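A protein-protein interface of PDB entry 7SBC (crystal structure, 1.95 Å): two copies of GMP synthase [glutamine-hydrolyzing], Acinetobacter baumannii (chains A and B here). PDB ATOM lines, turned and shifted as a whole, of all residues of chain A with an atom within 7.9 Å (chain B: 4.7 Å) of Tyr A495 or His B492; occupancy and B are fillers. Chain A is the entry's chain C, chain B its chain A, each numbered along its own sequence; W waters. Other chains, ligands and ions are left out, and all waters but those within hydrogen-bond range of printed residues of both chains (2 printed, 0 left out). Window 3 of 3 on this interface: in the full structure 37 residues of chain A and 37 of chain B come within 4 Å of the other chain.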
ATOM      1  N   HIS A 492     -15.601 -13.713  -5.783  1.00  0.00           N
ATOM      2  CA  HIS A 492     -16.425 -14.518  -6.689  1.00  0.00           C
ATOM      3  C   HIS A 492     -15.631 -14.972  -7.922  1.00  0.00           C
ATOM      4  O   HIS A 492     -16.007 -14.716  -9.068  1.00  0.00           O
ATOM      5  CB  HIS A 492     -17.642 -13.719  -7.150  1.00  0.00           C
ATOM      6  CG  HIS A 492     -18.625 -13.387  -6.072  1.00  0.00           C
ATOM      7  ND1 HIS A 492     -18.474 -12.303  -5.235  1.00  0.00           N
ATOM      8  CD2 HIS A 492     -19.805 -13.959  -5.738  1.00  0.00           C
ATOM      9  CE1 HIS A 492     -19.508 -12.234  -4.416  1.00  0.00           C
ATOM     10  NE2 HIS A 492     -20.331 -13.228  -4.700  1.00  0.00           N
ATOM     11  N   LEU A 493     -14.521 -15.663  -7.683  1.00  0.00           N
ATOM     12  CA  LEU A 493     -13.738 -16.178  -8.799  1.00  0.00           C
ATOM     13  C   LEU A 493     -14.510 -17.293  -9.500  1.00  0.00           C
ATOM     14  O   LEU A 493     -15.183 -18.091  -8.839  1.00  0.00           O
ATOM     15  CB  LEU A 493     -12.382 -16.698  -8.318  1.00  0.00           C
ATOM     16  CG  LEU A 493     -11.439 -15.714  -7.630  1.00  0.00           C
ATOM     17  CD1 LEU A 493     -10.164 -16.419  -7.173  1.00  0.00           C
ATOM     18  CD2 LEU A 493     -11.113 -14.535  -8.563  1.00  0.00           C
ATOM     19  N   PRO A 494     -14.448 -17.367 -10.832  1.00  0.00           N
ATOM     20  CA  PRO A 494     -15.163 -18.433 -11.545  1.00  0.00           C
ATOM     21  C   PRO A 494     -14.666 -19.810 -11.128  1.00  0.00           C
ATOM     22  O   PRO A 494     -13.469 -20.018 -10.904  1.00  0.00           O
ATOM     23  CB  PRO A 494     -14.853 -18.147 -13.019  1.00  0.00           C
ATOM     24  CG  PRO A 494     -14.534 -16.686 -13.055  1.00  0.00           C
ATOM     25  CD  PRO A 494     -13.860 -16.375 -11.752  1.00  0.00           C
ATOM     26  N   TYR A 495     -15.618 -20.745 -11.014  1.00  0.00           N
ATOM     27  CA  TYR A 495     -15.301 -22.134 -10.686  1.00  0.00           C
ATOM     28  C   TYR A 495     -14.140 -22.647 -11.525  1.00  0.00           C
ATOM     29  O   TYR A 495     -13.163 -23.192 -10.995  1.00  0.00           O
ATOM     30  CB  TYR A 495     -16.545 -23.018 -10.907  1.00  0.00           C
ATOM     31  CG  TYR A 495     -16.315 -24.499 -10.628  1.00  0.00           C
ATOM     32  CD1 TYR A 495     -15.696 -25.326 -11.566  1.00  0.00           C
ATOM     33  CD2 TYR A 495     -16.721 -25.066  -9.436  1.00  0.00           C
ATOM     34  CE1 TYR A 495     -15.476 -26.667 -11.311  1.00  0.00           C
ATOM     35  CE2 TYR A 495     -16.504 -26.415  -9.172  1.00  0.00           C
ATOM     36  CZ  TYR A 495     -15.882 -27.204 -10.117  1.00  0.00           C
ATOM     37  OH  TYR A 495     -15.670 -28.542  -9.860  1.00  0.00           O
ATOM     38  N   GLU A 496     -14.232 -22.487 -12.849  1.00  0.00           N
ATOM     39  CA  GLU A 496     -13.241 -23.117 -13.714  1.00  0.00           C
ATOM     40  C   GLU A 496     -11.877 -22.449 -13.601  1.00  0.00           C
ATOM     41  O   GLU A 496     -10.852 -23.108 -13.823  1.00  0.00           O
ATOM     42  CB  GLU A 496     -13.722 -23.120 -15.164  1.00  0.00           C
ATOM     43  CG  GLU A 496     -14.904 -24.057 -15.383  1.00  0.00           C
ATOM     44  CD  GLU A 496     -14.612 -25.532 -15.115  1.00  0.00           C
ATOM     45  OE1 GLU A 496     -13.428 -25.929 -15.007  1.00  0.00           O
ATOM     46  OE2 GLU A 496     -15.587 -26.309 -15.012  1.00  0.00           O
ATOM     47  N   LEU A 497     -11.840 -21.161 -13.249  1.00  0.00           N
ATOM     48  CA  LEU A 497     -10.559 -20.502 -13.019  1.00  0.00           C
ATOM     49  C   LEU A 497      -9.882 -21.042 -11.766  1.00  0.00           C
ATOM     50  O   LEU A 497      -8.675 -21.312 -11.767  1.00  0.00           O
ATOM     51  CB  LEU A 497     -10.755 -18.993 -12.901  1.00  0.00           C
ATOM     52  CG  LEU A 497      -9.492 -18.206 -12.529  1.00  0.00           C
ATOM     53  CD1 LEU A 497      -8.472 -18.286 -13.656  1.00  0.00           C
ATOM     54  CD2 LEU A 497      -9.825 -16.753 -12.232  1.00  0.00           C
ATOM     55  N   VAL A 498     -10.637 -21.165 -10.673  1.00  0.00           N
ATOM     56  CA  VAL A 498     -10.080 -21.730  -9.450  1.00  0.00           C
ATOM     57  C   VAL A 498      -9.618 -23.162  -9.689  1.00  0.00           C
ATOM     58  O   VAL A 498      -8.554 -23.570  -9.212  1.00  0.00           O
ATOM     59  CB  VAL A 498     -11.109 -21.639  -8.307  1.00  0.00           C
ATOM     60  CG1 VAL A 498     -10.584 -22.349  -7.059  1.00  0.00           C
ATOM     61  CG2 VAL A 498     -11.421 -20.181  -7.999  1.00  0.00           C
ATOM     62  N   ASP A 499     -10.392 -23.944 -10.444  1.00  0.00           N
ATOM     63  CA  ASP A 499      -9.968 -25.310 -10.733  1.00  0.00           C
ATOM     64  C   ASP A 499      -8.689 -25.332 -11.559  1.00  0.00           C
ATOM     65  O   ASP A 499      -7.831 -26.200 -11.361  1.00  0.00           O
ATOM     66  CB  ASP A 499     -11.061 -26.086 -11.457  1.00  0.00           C
ATOM     67  CG  ASP A 499     -10.729 -27.572 -11.557  1.00  0.00           C
ATOM     68  OD1 ASP A 499     -10.664 -28.230 -10.500  1.00  0.00           O
ATOM     69  OD2 ASP A 499     -10.500 -28.074 -12.677  1.00  0.00           O
ATOM     70  N   LYS A 500      -8.548 -24.397 -12.498  1.00  0.00           N
ATOM     71  CA  LYS A 500      -7.312 -24.332 -13.267  1.00  0.00           C
ATOM     72  C   LYS A 500      -6.131 -24.010 -12.366  1.00  0.00           C
ATOM     73  O   LYS A 500      -5.046 -24.573 -12.537  1.00  0.00           O
ATOM     74  CB  LYS A 500      -7.430 -23.295 -14.386  1.00  0.00           C
ATOM     75  CG  LYS A 500      -6.202 -23.252 -15.295  1.00  0.00           C
ATOM     76  CD  LYS A 500      -6.248 -22.080 -16.275  1.00  0.00           C
ATOM     77  CE  LYS A 500      -7.374 -22.217 -17.279  1.00  0.00           C
ATOM     78  NZ  LYS A 500      -7.441 -21.048 -18.208  1.00  0.00           N
ATOM     79  N   ILE A 501      -6.328 -23.114 -11.392  1.00  0.00           N
ATOM     80  CA  ILE A 501      -5.238 -22.701 -10.512  1.00  0.00           C
ATOM     81  C   ILE A 501      -4.803 -23.854  -9.612  1.00  0.00           C
ATOM     82  O   ILE A 501      -3.603 -24.114  -9.442  1.00  0.00           O
ATOM     83  CB  ILE A 501      -5.655 -21.479  -9.678  1.00  0.00           C
ATOM     84  CG1 ILE A 501      -5.897 -20.260 -10.582  1.00  0.00           C
ATOM     85  CG2 ILE A 501      -4.588 -21.179  -8.617  1.00  0.00           C
ATOM     86  CD1 ILE A 501      -6.715 -19.161  -9.911  1.00  0.00           C
ATOM     87  N   SER A 502      -5.767 -24.548  -8.999  1.00  0.00           N
ATOM     88  CA  SER A 502      -5.394 -25.625  -8.088  1.00  0.00           C
ATOM     89  C   SER A 502      -4.757 -26.781  -8.845  1.00  0.00           C
ATOM     90  O   SER A 502      -3.761 -27.353  -8.388  1.00  0.00           O
ATOM     91  CB  SER A 502      -6.601 -26.100  -7.273  1.00  0.00           C
ATOM     92  OG  SER A 502      -7.598 -26.675  -8.092  1.00  0.00           O
ATOM     93  N   TRP B 445     -28.864 -28.983  -0.717  1.00  0.00           N
ATOM     94  CA  TRP B 445     -27.631 -29.291  -1.423  1.00  0.00           C
ATOM     95  C   TRP B 445     -26.938 -30.557  -0.915  1.00  0.00           C
ATOM     96  O   TRP B 445     -26.000 -31.026  -1.570  1.00  0.00           O
ATOM     97  CB  TRP B 445     -26.676 -28.079  -1.365  1.00  0.00           C
ATOM     98  CG  TRP B 445     -27.105 -27.049  -2.380  1.00  0.00           C
ATOM     99  CD1 TRP B 445     -28.036 -26.067  -2.209  1.00  0.00           C
ATOM    100  CD2 TRP B 445     -26.692 -26.979  -3.748  1.00  0.00           C
ATOM    101  NE1 TRP B 445     -28.214 -25.372  -3.384  1.00  0.00           N
ATOM    102  CE2 TRP B 445     -27.395 -25.910  -4.343  1.00  0.00           C
ATOM    103  CE3 TRP B 445     -25.787 -27.708  -4.528  1.00  0.00           C
ATOM    104  CZ2 TRP B 445     -27.216 -25.549  -5.676  1.00  0.00           C
ATOM    105  CZ3 TRP B 445     -25.608 -27.346  -5.850  1.00  0.00           C
ATOM    106  CH2 TRP B 445     -26.322 -26.274  -6.412  1.00  0.00           C
ATOM    107  N   GLU B 481     -18.479 -33.786  -6.294  1.00  0.00           N
ATOM    108  CA  GLU B 481     -19.444 -34.343  -7.226  1.00  0.00           C
ATOM    109  C   GLU B 481     -18.749 -35.478  -7.959  1.00  0.00           C
ATOM    110  O   GLU B 481     -17.647 -35.294  -8.487  1.00  0.00           O
ATOM    111  CB  GLU B 481     -19.937 -33.282  -8.225  1.00  0.00           C
ATOM    112  CG  GLU B 481     -20.675 -32.105  -7.586  1.00  0.00           C
ATOM    113  CD  GLU B 481     -20.592 -30.802  -8.405  1.00  0.00           C
ATOM    114  OE1 GLU B 481     -20.016 -30.798  -9.512  1.00  0.00           O
ATOM    115  OE2 GLU B 481     -21.115 -29.774  -7.931  1.00  0.00           O
ATOM    116  N   ARG B 489     -14.929 -33.990  -8.917  1.00  0.00           N
ATOM    117  CA  ARG B 489     -14.674 -32.560  -8.976  1.00  0.00           C
ATOM    118  C   ARG B 489     -15.160 -31.921  -7.686  1.00  0.00           C
ATOM    119  O   ARG B 489     -16.105 -32.409  -7.061  1.00  0.00           O
ATOM    120  CB  ARG B 489     -15.378 -31.917 -10.171  1.00  0.00           C
ATOM    121  CG  ARG B 489     -14.994 -32.517 -11.514  1.00  0.00           C
ATOM    122  CD  ARG B 489     -15.347 -31.560 -12.659  1.00  0.00           C
ATOM    123  NE  ARG B 489     -14.331 -30.529 -12.863  1.00  0.00           N
ATOM    124  CZ  ARG B 489     -14.497 -29.452 -13.623  1.00  0.00           C
ATOM    125  NH1 ARG B 489     -15.646 -29.205 -14.233  1.00  0.00           N
ATOM    126  NH2 ARG B 489     -13.486 -28.602 -13.775  1.00  0.00           N
ATOM    127  N   PHE B 490     -14.513 -30.835  -7.269  1.00  0.00           N
ATOM    128  CA  PHE B 490     -15.014 -30.151  -6.086  1.00  0.00           C
ATOM    129  C   PHE B 490     -16.370 -29.529  -6.415  1.00  0.00           C
ATOM    130  O   PHE B 490     -16.627 -29.140  -7.558  1.00  0.00           O
ATOM    131  CB  PHE B 490     -13.988 -29.136  -5.552  1.00  0.00           C
ATOM    132  CG  PHE B 490     -13.815 -27.877  -6.381  1.00  0.00           C
ATOM    133  CD1 PHE B 490     -14.592 -26.757  -6.128  1.00  0.00           C
ATOM    134  CD2 PHE B 490     -12.806 -27.785  -7.329  1.00  0.00           C
ATOM    135  CE1 PHE B 490     -14.404 -25.576  -6.848  1.00  0.00           C
ATOM    136  CE2 PHE B 490     -12.618 -26.610  -8.059  1.00  0.00           C
ATOM    137  CZ  PHE B 490     -13.419 -25.512  -7.819  1.00  0.00           C
ATOM    138  N   ALA B 491     -17.271 -29.516  -5.429  1.00  0.00           N
ATOM    139  CA  ALA B 491     -18.683 -29.284  -5.713  1.00  0.00           C
ATOM    140  C   ALA B 491     -18.970 -27.824  -6.061  1.00  0.00           C
ATOM    141  O   ALA B 491     -18.352 -26.899  -5.524  1.00  0.00           O
ATOM    142  CB  ALA B 491     -19.550 -29.694  -4.528  1.00  0.00           C
ATOM    143  N   HIS B 492     -19.953 -27.635  -6.949  1.00  0.00           N
ATOM    144  CA  HIS B 492     -20.417 -26.313  -7.384  1.00  0.00           C
ATOM    145  C   HIS B 492     -21.420 -25.729  -6.385  1.00  0.00           C
ATOM    146  O   HIS B 492     -22.544 -25.368  -6.736  1.00  0.00           O
ATOM    147  CB  HIS B 492     -21.073 -26.394  -8.759  1.00  0.00           C
ATOM    148  CG  HIS B 492     -20.137 -26.694  -9.889  1.00  0.00           C
ATOM    149  ND1 HIS B 492     -19.699 -27.970 -10.176  1.00  0.00           N
ATOM    150  CD2 HIS B 492     -19.594 -25.887 -10.830  1.00  0.00           C
ATOM    151  CE1 HIS B 492     -18.910 -27.933 -11.236  1.00  0.00           C
ATOM    152  NE2 HIS B 492     -18.826 -26.680 -11.649  1.00  0.00           N
ATOM    153  N   LEU B 493     -21.014 -25.660  -5.128  1.00  0.00           N
ATOM    154  CA  LEU B 493     -21.887 -25.093  -4.108  1.00  0.00           C
ATOM    155  C   LEU B 493     -22.090 -23.597  -4.354  1.00  0.00           C
ATOM    156  O   LEU B 493     -21.131 -22.885  -4.669  1.00  0.00           O
ATOM    157  CB  LEU B 493     -21.297 -25.315  -2.715  1.00  0.00           C
ATOM    158  CG  LEU B 493     -21.160 -26.773  -2.251  1.00  0.00           C
ATOM    159  CD1 LEU B 493     -20.512 -26.840  -0.863  1.00  0.00           C
ATOM    160  CD2 LEU B 493     -22.532 -27.458  -2.258  1.00  0.00           C
ATOM    161  N   PRO B 494     -23.319 -23.090  -4.203  1.00  0.00           N
ATOM    162  CA  PRO B 494     -23.552 -21.651  -4.397  1.00  0.00           C
ATOM    163  C   PRO B 494     -22.704 -20.819  -3.449  1.00  0.00           C
ATOM    164  O   PRO B 494     -22.500 -21.180  -2.288  1.00  0.00           O
ATOM    165  CB  PRO B 494     -25.047 -21.484  -4.099  1.00  0.00           C
ATOM    166  CG  PRO B 494     -25.635 -22.826  -4.363  1.00  0.00           C
ATOM    167  CD  PRO B 494     -24.571 -23.820  -3.942  1.00  0.00           C
ATOM    168  N   SER B 521      -9.632 -31.203  -7.214  1.00  0.00           N
ATOM    169  CA  SER B 521     -10.396 -32.317  -7.747  1.00  0.00           C
ATOM    170  C   SER B 521      -9.578 -33.606  -7.701  1.00  0.00           C
ATOM    171  O   SER B 521      -8.363 -33.601  -7.497  1.00  0.00           O
ATOM    172  CB  SER B 521     -10.852 -32.013  -9.176  1.00  0.00           C
ATOM    173  OG  SER B 521     -11.719 -30.882  -9.201  1.00  0.00           O
HETATM  174  O   HOH W   1      -8.480 -29.112  -8.991  1.00  0.00           O
HETATM  175  O   HOH W   2     -17.955 -25.956 -14.073  1.00  0.00           O
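The side-chain carboxylate of Glu A496 is in salt-bridge range of the guanidinium group of Arg B489 (2.9 Å).
The side-chain carboxylate of Asp A499 lies within salt-bridge range of the guanidinium group of Arg B489, 3.2 Å away.
The side-chain hydroxyl of Tyr A495 is in hydrogen-bond range of the backbone carbonyl oxygen of Phe B490 (2.6 Å).
The side-chain carboxylate (OD1) of Asp A499 sits at hydrogen-bond distance from the side-chain hydroxyl (OG) of Ser B521.
The backbone carbonyl oxygen of Asp A499 lies within hydrogen-bond range of the side-chain hydroxyl of Ser A502.
The backbone NH (N) of Phe B490 sits at hydrogen-bond distance from the side-chain hydroxyl (OG) of Ser B521 (3.4 Å).
N of Glu B481 sits at hydrogen-bond distance from O of Arg B489 (2.8 Å).
OE2 of Glu B481 is in hydrogen-bond range of N of His B492 (2.6 Å).
Among the printed residues, pairs that only touch across the chains: Tyr A495 with Arg B489, Tyr A495 with His B492 and Asp A499 with Phe B490.
Tyr A495 touches three residues of chain B.
Printed residues of chain B within 4 Å of Glu A496: Arg B489.
Of the printed residues of chain B, Asp A499 touches Arg B489 (3.2 Å), Phe B490 (3.5 Å) and Ser B521 (3.1 Å).
Printed residues of chain A within 4 Å of Arg B489: Tyr A495, Glu A496 and Asp A499.
The nearest residue of chain B that does not touch Tyr A495 is Ala B491 (4.1 Å).
Of the 9 printed residues of chain B, 4 touch a printed residue of chain A.
Printed residues of chain B that touch a printed residue of chain A: Arg B489, Phe B490, His B492 and Ser B521.
Positions printed for both chains: 492, 493 and 494.
Water W2 bridges OE2 of Glu A496 (2.6 Å) and NE2 of His B492 (2.7 Å).
Water W1 lies within hydrogen-bond range of OG of Ser A502 (2.7 Å), OD1 of Asp A499 (2.8 Å) and N of Ser B521 (3.0 Å).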
